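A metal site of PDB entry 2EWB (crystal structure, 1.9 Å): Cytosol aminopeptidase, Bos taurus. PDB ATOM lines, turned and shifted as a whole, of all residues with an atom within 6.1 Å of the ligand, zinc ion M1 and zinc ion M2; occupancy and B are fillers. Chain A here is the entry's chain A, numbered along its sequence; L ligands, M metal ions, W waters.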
ATOM      1  N   LYS A 250       5.865  18.361  18.207  1.00  0.00           N
ATOM      2  CA  LYS A 250       5.877  17.662  16.928  1.00  0.00           C
ATOM      3  C   LYS A 250       7.290  17.143  16.716  1.00  0.00           C
ATOM      4  O   LYS A 250       8.241  17.923  16.649  1.00  0.00           O
ATOM      5  CB  LYS A 250       5.499  18.625  15.803  1.00  0.00           C
ATOM      6  CG  LYS A 250       5.739  18.077  14.398  1.00  0.00           C
ATOM      7  CD  LYS A 250       5.433  19.142  13.327  1.00  0.00           C
ATOM      8  CE  LYS A 250       5.777  18.627  11.936  1.00  0.00           C
ATOM      9  NZ  LYS A 250       5.493  19.633  10.874  1.00  0.00           N
ATOM     10  N   ILE A 252       8.819  15.273  14.017  1.00  0.00           N
ATOM     11  CA  ILE A 252       9.102  14.687  12.708  1.00  0.00           C
ATOM     12  C   ILE A 252      10.615  14.864  12.521  1.00  0.00           C
ATOM     13  O   ILE A 252      11.077  15.968  12.222  1.00  0.00           O
ATOM     14  CB  ILE A 252       8.330  15.409  11.590  1.00  0.00           C
ATOM     15  CG1 ILE A 252       6.821  15.206  11.789  1.00  0.00           C
ATOM     16  CG2 ILE A 252       8.757  14.875  10.230  1.00  0.00           C
ATOM     17  CD1 ILE A 252       6.362  13.760  11.631  1.00  0.00           C
ATOM     18  N   ASP A 255      11.181  15.417   7.410  1.00  0.00           N
ATOM     19  CA  ASP A 255       9.967  15.515   6.635  1.00  0.00           C
ATOM     20  C   ASP A 255      10.244  15.742   5.158  1.00  0.00           C
ATOM     21  O   ASP A 255      10.689  16.817   4.754  1.00  0.00           O
ATOM     22  CB  ASP A 255       9.106  16.641   7.186  1.00  0.00           C
ATOM     23  CG  ASP A 255       7.751  16.711   6.530  1.00  0.00           C
ATOM     24  OD1 ASP A 255       7.349  15.716   5.897  1.00  0.00           O
ATOM     25  OD2 ASP A 255       7.088  17.746   6.669  1.00  0.00           O
ATOM     26  N   GLY A 257       7.816  15.276   3.155  1.00  0.00           N
ATOM     27  CA  GLY A 257       6.480  15.612   2.703  1.00  0.00           C
ATOM     28  C   GLY A 257       5.690  14.336   2.435  1.00  0.00           C
ATOM     29  O   GLY A 257       4.463  14.333   2.433  1.00  0.00           O
ATOM     30  N   LYS A 262       7.882  17.227  -0.917  1.00  0.00           N
ATOM     31  CA  LYS A 262       8.363  18.602  -0.913  1.00  0.00           C
ATOM     32  C   LYS A 262       9.307  18.857  -2.081  1.00  0.00           C
ATOM     33  O   LYS A 262       9.834  17.917  -2.683  1.00  0.00           O
ATOM     34  CB  LYS A 262       9.125  18.907   0.370  1.00  0.00           C
ATOM     35  CG  LYS A 262       8.276  18.907   1.622  1.00  0.00           C
ATOM     36  CD  LYS A 262       9.160  19.089   2.847  1.00  0.00           C
ATOM     37  CE  LYS A 262       8.313  19.213   4.101  1.00  0.00           C
ATOM     38  NZ  LYS A 262       7.446  20.407   4.023  1.00  0.00           N
ATOM     39  N   MET A 270      14.372  20.396   6.834  1.00  0.00           N
ATOM     40  CA  MET A 270      13.295  19.616   7.429  1.00  0.00           C
ATOM     41  C   MET A 270      13.815  18.613   8.453  1.00  0.00           C
ATOM     42  O   MET A 270      13.033  17.863   9.049  1.00  0.00           O
ATOM     43  CB  MET A 270      12.467  18.930   6.350  1.00  0.00           C
ATOM     44  CG  MET A 270      11.704  19.894   5.456  1.00  0.00           C
ATOM     45  SD  MET A 270      10.850  21.200   6.380  1.00  0.00           S
ATOM     46  CE  MET A 270       9.697  20.264   7.304  1.00  0.00           C
ATOM     47  N   ASP A 273      12.261  19.489  11.603  1.00  0.00           N
ATOM     48  CA  ASP A 273      10.812  19.424  11.702  1.00  0.00           C
ATOM     49  C   ASP A 273      10.407  18.749  13.001  1.00  0.00           C
ATOM     50  O   ASP A 273       9.239  18.439  13.229  1.00  0.00           O
ATOM     51  CB  ASP A 273      10.239  18.679  10.494  1.00  0.00           C
ATOM     52  CG  ASP A 273       8.792  19.048  10.212  1.00  0.00           C
ATOM     53  OD1 ASP A 273       8.398  20.202  10.498  1.00  0.00           O
ATOM     54  OD2 ASP A 273       8.048  18.199   9.679  1.00  0.00           O
ATOM     55  N   ASN A 305       8.677  11.296   7.902  1.00  0.00           N
ATOM     56  CA  ASN A 305       7.579  11.345   6.944  1.00  0.00           C
ATOM     57  C   ASN A 305       8.268  11.099   5.621  1.00  0.00           C
ATOM     58  O   ASN A 305       8.887  11.996   5.050  1.00  0.00           O
ATOM     59  CB  ASN A 305       6.876  12.699   6.966  1.00  0.00           C
ATOM     60  CG  ASN A 305       5.619  12.715   6.124  1.00  0.00           C
ATOM     61  OD1 ASN A 305       4.986  11.676   5.908  1.00  0.00           O
ATOM     62  ND2 ASN A 305       5.231  13.891   5.658  1.00  0.00           N
ATOM     63  N   ASN A 330      -3.307  16.009   2.185  1.00  0.00           N
ATOM     64  CA  ASN A 330      -1.928  16.353   1.899  1.00  0.00           C
ATOM     65  C   ASN A 330      -1.052  15.683   2.955  1.00  0.00           C
ATOM     66  O   ASN A 330      -1.111  16.024   4.130  1.00  0.00           O
ATOM     67  CB  ASN A 330      -1.740  17.863   1.919  1.00  0.00           C
ATOM     68  CG  ASN A 330      -0.357  18.276   1.469  1.00  0.00           C
ATOM     69  OD1 ASN A 330       0.644  17.771   1.970  1.00  0.00           O
ATOM     70  ND2 ASN A 330      -0.287  19.223   0.532  1.00  0.00           N
ATOM     71  N   THR A 331      -0.249  14.726   2.517  1.00  0.00           N
ATOM     72  CA  THR A 331       0.606  13.984   3.429  1.00  0.00           C
ATOM     73  C   THR A 331       1.725  14.821   4.038  1.00  0.00           C
ATOM     74  O   THR A 331       2.415  14.363   4.938  1.00  0.00           O
ATOM     75  CB  THR A 331       1.233  12.761   2.743  1.00  0.00           C
ATOM     76  OG1 THR A 331       2.186  13.203   1.755  1.00  0.00           O
ATOM     77  CG2 THR A 331       0.149  11.933   2.049  1.00  0.00           C
ATOM     78  N   ASP A 332       1.896  16.041   3.528  1.00  0.00           N
ATOM     79  CA  ASP A 332       2.940  16.912   4.044  1.00  0.00           C
ATOM     80  C   ASP A 332       2.397  17.758   5.201  1.00  0.00           C
ATOM     81  O   ASP A 332       3.120  18.555   5.796  1.00  0.00           O
ATOM     82  CB  ASP A 332       3.492  17.806   2.926  1.00  0.00           C
ATOM     83  CG  ASP A 332       4.803  18.479   3.300  1.00  0.00           C
ATOM     84  OD1 ASP A 332       5.401  18.095   4.334  1.00  0.00           O
ATOM     85  OD2 ASP A 332       5.236  19.377   2.553  1.00  0.00           O
ATOM     86  N   ALA A 333       1.111  17.590   5.503  1.00  0.00           N
ATOM     87  CA  ALA A 333       0.503  18.279   6.632  1.00  0.00           C
ATOM     88  C   ALA A 333       0.444  17.150   7.675  1.00  0.00           C
ATOM     89  O   ALA A 333      -0.611  16.834   8.207  1.00  0.00           O
ATOM     90  CB  ALA A 333      -0.902  18.745   6.284  1.00  0.00           C
ATOM     91  N   GLU A 334       1.603  16.560   7.929  1.00  0.00           N
ATOM     92  CA  GLU A 334       1.714  15.426   8.841  1.00  0.00           C
ATOM     93  C   GLU A 334       1.881  15.772  10.313  1.00  0.00           C
ATOM     94  O   GLU A 334       1.574  14.960  11.181  1.00  0.00           O
ATOM     95  CB  GLU A 334       2.863  14.505   8.404  1.00  0.00           C
ATOM     96  CG  GLU A 334       4.263  14.921   8.892  1.00  0.00           C
ATOM     97  CD  GLU A 334       4.717  16.297   8.415  1.00  0.00           C
ATOM     98  OE1 GLU A 334       4.430  16.643   7.259  1.00  0.00           O
ATOM     99  OE2 GLU A 334       5.371  17.011   9.207  1.00  0.00           O
ATOM    100  N   GLY A 335       2.387  16.965  10.584  1.00  0.00           N
ATOM    101  CA  GLY A 335       2.590  17.371  11.961  1.00  0.00           C
ATOM    102  C   GLY A 335       1.294  17.419  12.740  1.00  0.00           C
ATOM    103  O   GLY A 335       1.237  16.980  13.897  1.00  0.00           O
ATOM    104  N   ARG A 336       0.231  17.925  12.121  1.00  0.00           N
ATOM    105  CA  ARG A 336      -1.043  17.997  12.805  1.00  0.00           C
ATOM    106  C   ARG A 336      -1.616  16.594  13.003  1.00  0.00           C
ATOM    107  O   ARG A 336      -2.375  16.353  13.934  1.00  0.00           O
ATOM    108  CB  ARG A 336      -2.021  18.892  12.039  1.00  0.00           C
ATOM    109  CG  ARG A 336      -2.452  18.374  10.682  1.00  0.00           C
ATOM    110  CD  ARG A 336      -3.051  19.521   9.865  1.00  0.00           C
ATOM    111  NE  ARG A 336      -2.002  20.404   9.353  1.00  0.00           N
ATOM    112  CZ  ARG A 336      -2.227  21.510   8.647  1.00  0.00           C
ATOM    113  NH1 ARG A 336      -3.465  21.898   8.391  1.00  0.00           N
ATOM    114  NH2 ARG A 336      -1.201  22.217   8.193  1.00  0.00           N
ATOM    115  N   THR A 359       6.861  22.932  14.371  1.00  0.00           N
ATOM    116  CA  THR A 359       7.314  23.662  13.196  1.00  0.00           C
ATOM    117  C   THR A 359       6.177  23.262  12.267  1.00  0.00           C
ATOM    118  O   THR A 359       6.363  22.498  11.313  1.00  0.00           O
ATOM    119  CB  THR A 359       8.634  23.093  12.697  1.00  0.00           C
ATOM    120  OG1 THR A 359       8.551  21.667  12.681  1.00  0.00           O
ATOM    121  CG2 THR A 359       9.780  23.519  13.607  1.00  0.00           C
ATOM    122  N   LEU A 360       4.999  23.784  12.555  1.00  0.00           N
ATOM    123  CA  LEU A 360       3.799  23.399  11.838  1.00  0.00           C
ATOM    124  C   LEU A 360       3.470  23.932  10.454  1.00  0.00           C
ATOM    125  O   LEU A 360       3.022  23.168   9.616  1.00  0.00           O
ATOM    126  CB  LEU A 360       2.587  23.619  12.745  1.00  0.00           C
ATOM    127  CG  LEU A 360       1.371  22.733  12.458  1.00  0.00           C
ATOM    128  CD1 LEU A 360       1.736  21.266  12.719  1.00  0.00           C
ATOM    129  CD2 LEU A 360       0.221  23.156  13.350  1.00  0.00           C
ATOM    130  N   THR A 361       3.665  25.213  10.204  1.00  0.00           N
ATOM    131  CA  THR A 361       3.280  25.714   8.886  1.00  0.00           C
ATOM    132  C   THR A 361       4.210  26.737   8.279  1.00  0.00           C
ATOM    133  O   THR A 361       4.806  27.563   8.972  1.00  0.00           O
ATOM    134  CB  THR A 361       1.880  26.355   8.925  1.00  0.00           C
ATOM    135  OG1 THR A 361       1.916  27.534   9.748  1.00  0.00           O
ATOM    136  CG2 THR A 361       0.852  25.379   9.496  1.00  0.00           C
ATOM    137  N   GLY A 362       4.337  26.680   6.953  1.00  0.00           N
ATOM    138  CA  GLY A 362       5.162  27.643   6.253  1.00  0.00           C
ATOM    139  C   GLY A 362       4.387  28.948   6.332  1.00  0.00           C
ATOM    140  O   GLY A 362       4.948  30.030   6.261  1.00  0.00           O
ATOM    141  N   ALA A 363       3.075  28.822   6.496  1.00  0.00           N
ATOM    142  CA  ALA A 363       2.210  30.000   6.595  1.00  0.00           C
ATOM    143  C   ALA A 363       2.617  30.850   7.789  1.00  0.00           C
ATOM    144  O   ALA A 363       2.538  32.076   7.736  1.00  0.00           O
ATOM    145  CB  ALA A 363       0.753  29.571   6.727  1.00  0.00           C
ATOM    146  N   ASN A 420      -7.130  17.336   6.917  1.00  0.00           N
ATOM    147  CA  ASN A 420      -5.850  17.798   7.442  1.00  0.00           C
ATOM    148  C   ASN A 420      -5.286  19.041   6.749  1.00  0.00           C
ATOM    149  O   ASN A 420      -4.164  19.461   7.046  1.00  0.00           O
ATOM    150  CB  ASN A 420      -4.830  16.644   7.489  1.00  0.00           C
ATOM    151  CG  ASN A 420      -4.091  16.436   6.185  1.00  0.00           C
ATOM    152  OD1 ASN A 420      -4.660  16.553   5.097  1.00  0.00           O
ATOM    153  ND2 ASN A 420      -2.814  16.092   6.286  1.00  0.00           N
ATOM    154  N   ILE A 421      -6.061  19.613   5.832  1.00  0.00           N
ATOM    155  CA  ILE A 421      -5.679  20.856   5.167  1.00  0.00           C
ATOM    156  C   ILE A 421      -6.969  21.640   4.938  1.00  0.00           C
ATOM    157  O   ILE A 421      -8.018  21.062   4.663  1.00  0.00           O
ATOM    158  CB  ILE A 421      -4.969  20.639   3.804  1.00  0.00           C
ATOM    159  CG1 ILE A 421      -5.905  19.946   2.811  1.00  0.00           C
ATOM    160  CG2 ILE A 421      -3.691  19.875   4.010  1.00  0.00           C
ATOM    161  CD1 ILE A 421      -5.365  19.933   1.389  1.00  0.00           C
ATOM    162  N   GLY A 422      -6.896  22.966   5.075  1.00  0.00           N
ATOM    163  CA  GLY A 422      -8.068  23.790   4.894  1.00  0.00           C
ATOM    164  C   GLY A 422      -8.584  23.754   3.471  1.00  0.00           C
ATOM    165  O   GLY A 422      -7.855  23.373   2.556  1.00  0.00           O
ATOM    166  N   TYR A 424      -9.317  26.286   1.784  1.00  0.00           N
ATOM    167  CA  TYR A 424      -8.717  27.437   1.119  1.00  0.00           C
ATOM    168  C   TYR A 424      -7.239  27.441   1.517  1.00  0.00           C
ATOM    169  O   TYR A 424      -6.854  26.830   2.512  1.00  0.00           O
ATOM    170  CB  TYR A 424      -9.391  28.740   1.565  1.00  0.00           C
ATOM    171  CG  TYR A 424     -10.896  28.773   1.391  1.00  0.00           C
ATOM    172  CD1 TYR A 424     -11.497  28.374   0.193  1.00  0.00           C
ATOM    173  CD2 TYR A 424     -11.719  29.199   2.429  1.00  0.00           C
ATOM    174  CE1 TYR A 424     -12.883  28.420   0.036  1.00  0.00           C
ATOM    175  CE2 TYR A 424     -13.108  29.248   2.280  1.00  0.00           C
ATOM    176  CZ  TYR A 424     -13.687  28.850   1.077  1.00  0.00           C
ATOM    177  OH  TYR A 424     -15.052  28.882   0.931  1.00  0.00           O
ATOM    178  N   ARG A 425      -6.409  28.122   0.739  1.00  0.00           N
ATOM    179  CA  ARG A 425      -4.982  28.166   1.026  1.00  0.00           C
ATOM    180  C   ARG A 425      -4.607  29.306   1.971  1.00  0.00           C
ATOM    181  O   ARG A 425      -3.460  29.427   2.384  1.00  0.00           O
ATOM    182  CB  ARG A 425      -4.192  28.287  -0.283  1.00  0.00           C
ATOM    183  N   ALA A 451       7.485  27.310  13.255  1.00  0.00           N
ATOM    184  CA  ALA A 451       8.071  27.141  11.936  1.00  0.00           C
ATOM    185  C   ALA A 451       8.885  28.364  11.502  1.00  0.00           C
ATOM    186  O   ALA A 451       9.941  28.228  10.887  1.00  0.00           O
ATOM    187  CB  ALA A 451       6.981  26.845  10.907  1.00  0.00           C
HETATM  188  C1  LIG L   1      -2.071  22.915   2.608  1.00  0.00           C
HETATM  189  C2  LIG L   1      -0.751  23.363   2.463  1.00  0.00           C
HETATM  190  C3  LIG L   1      -0.242  23.581   1.157  1.00  0.00           C
HETATM  191  C4  LIG L   1      -1.047  23.351   0.019  1.00  0.00           C
HETATM  192  C5  LIG L   1      -2.379  22.904   0.172  1.00  0.00           C
HETATM  193  C6  LIG L   1      -2.899  22.693   1.472  1.00  0.00           C
HETATM  194  C7  LIG L   1       2.907  21.652   3.409  1.00  0.00           C
HETATM  195  C8  LIG L   1       3.184  22.798   2.408  1.00  0.00           C
HETATM  196  C9  LIG L   1       1.486  21.092   3.327  1.00  0.00           C
HETATM  197  C10 LIG L   1       0.729  21.919   4.365  1.00  0.00           C
HETATM  198  C11 LIG L   1       1.711  21.872   5.504  1.00  0.00           C
HETATM  199  C12 LIG L   1       5.541  23.483   7.136  1.00  0.00           C
HETATM  200  C13 LIG L   1       4.389  22.487   6.858  1.00  0.00           C
HETATM  201  C14 LIG L   1       4.266  22.147   5.361  1.00  0.00           C
HETATM  202  C15 LIG L   1       4.548  21.249   7.750  1.00  0.00           C
HETATM  203  O1  LIG L   1       3.162  22.564   1.198  1.00  0.00           O
HETATM  204  O2  LIG L   1       3.434  23.926   2.850  1.00  0.00           O
HETATM  205  O3  LIG L   1       5.288  21.986   4.680  1.00  0.00           O
HETATM  206  N1  LIG L   1       3.023  22.043   4.825  1.00  0.00           N
HETATM  207  S1  LIG L   1       0.290  23.633   3.919  1.00  0.00           S
HETATM  208  S2  LIG L   1       5.859  20.122   7.302  1.00  0.00           S
HETATM  209 ZN    ZN M   1       5.184  18.200   6.278  1.00  0.00          ZN
HETATM  210 ZN    ZN M   2       6.274  18.822   9.160  1.00  0.00          ZN
HETATM  211  O   HOH W   1      -1.067  21.616  -2.977  1.00  0.00           O
HETATM  212  O   HOH W   2      -3.834  25.157   4.120  1.00  0.00           O
HETATM  213  O   HOH W   3       2.941  25.057   5.339  1.00  0.00           O
HETATM  214  O   HOH W   4      -1.537  26.737   0.426  1.00  0.00           O
HETATM  215  O   HOH W   5       0.560  26.488   5.682  1.00  0.00           O
HETATM  216  O   HOH W   6       2.235  20.490  -0.258  1.00  0.00           O
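Zinc ion M2 is bound by OD2 of Asp 273, at 2.0 Å. Zinc ion M2 is bound by OE2 of Glu 334 (2.0 Å). NZ of Lys 250 binds zinc ion M2. S2 of the ligand binds zinc ion M2 (2.3 Å). Zinc ion M2 has four donor atoms within binding distance. Slightly farther from zinc ion M2 lies OD2 of Asp 255 (2.8 Å).
Water W6 lies within hydrogen-bond range of O1 of the ligand (2.7 Å) and ND2 of Asn 330 (2.9 Å). Water W3 bridges the backbone NH (N) of Gly 362 (2.7 Å) and an oxygen (O2) of the ligand (2.8 Å).
Merely in contact with the ligand: Leu 360, Gly 362, Thr 361, Asn 330, Ile 421, Met 270, Ala 333 and Arg 336. Hydrophobic or aromatic side chains within 4 Å of the ligand: Met 270 and Ile 421. Within 4 Å of the ligand: Lys 250, Asp 255, Lys 262, Met 270, Asp 273, Asn 330, Asp 332, Ala 333, Glu 334, Arg 336, Leu 360, Thr 361, Gly 362 and Ile 421. The nearest printed residue that does not touch the ligand is Thr 359 (4.2 Å).
N of Ile 252 is in hydrogen-bond range of O of Asp 273. The side-chain amino group (NZ) of Lys 262 is in salt-bridge range of the side-chain carboxylate (OD2) of Asp 332. N of Asp 332 is in hydrogen-bond range of OD1 of Asn 330 (2.6 Å). The backbone NH (N) of Asp 332 is in hydrogen-bond range of the backbone carbonyl oxygen (O) of Gly 257. ND2 of Asn 305 lies close to OE1 of Glu 334. The backbone NH of Asp 255 is in hydrogen-bond range of the backbone carbonyl oxygen of Met 270. The side-chain carboxylate (OD1) of Asp 255 is in hydrogen-bond range of the backbone NH (N) of Gly 257, at 2.8 Å. O of Asn 330 lies within hydrogen-bond range of ND2 of Asn 420 (2.7 Å).
The side-chain amino group (NZ) of Lys 262 sits at hydrogen-bond distance from an oxygen (O3) of the ligand, 2.8 Å away.
Zinc ion M1 is bound by the side-chain carboxylate (OD1) of Asp 332 (2.0 Å), the side-chain carboxylate (OE1) of Glu 334 (2.0 Å), the side-chain carboxylate (OD2) of Asp 255 (2.0 Å), the backbone carbonyl oxygen (O) of Asp 332 (2.1 Å) and a sulfur (S2) of the ligand (2.3 Å).
Within 4 Å of zinc ion M2: Lys 250, Asp 255, Asp 273 and Glu 334.
Merely in contact with zinc ion M1: Lys 262. Within 4 Å of zinc ion M1: Asp 255, Lys 262, Asp 332 and Glu 334.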
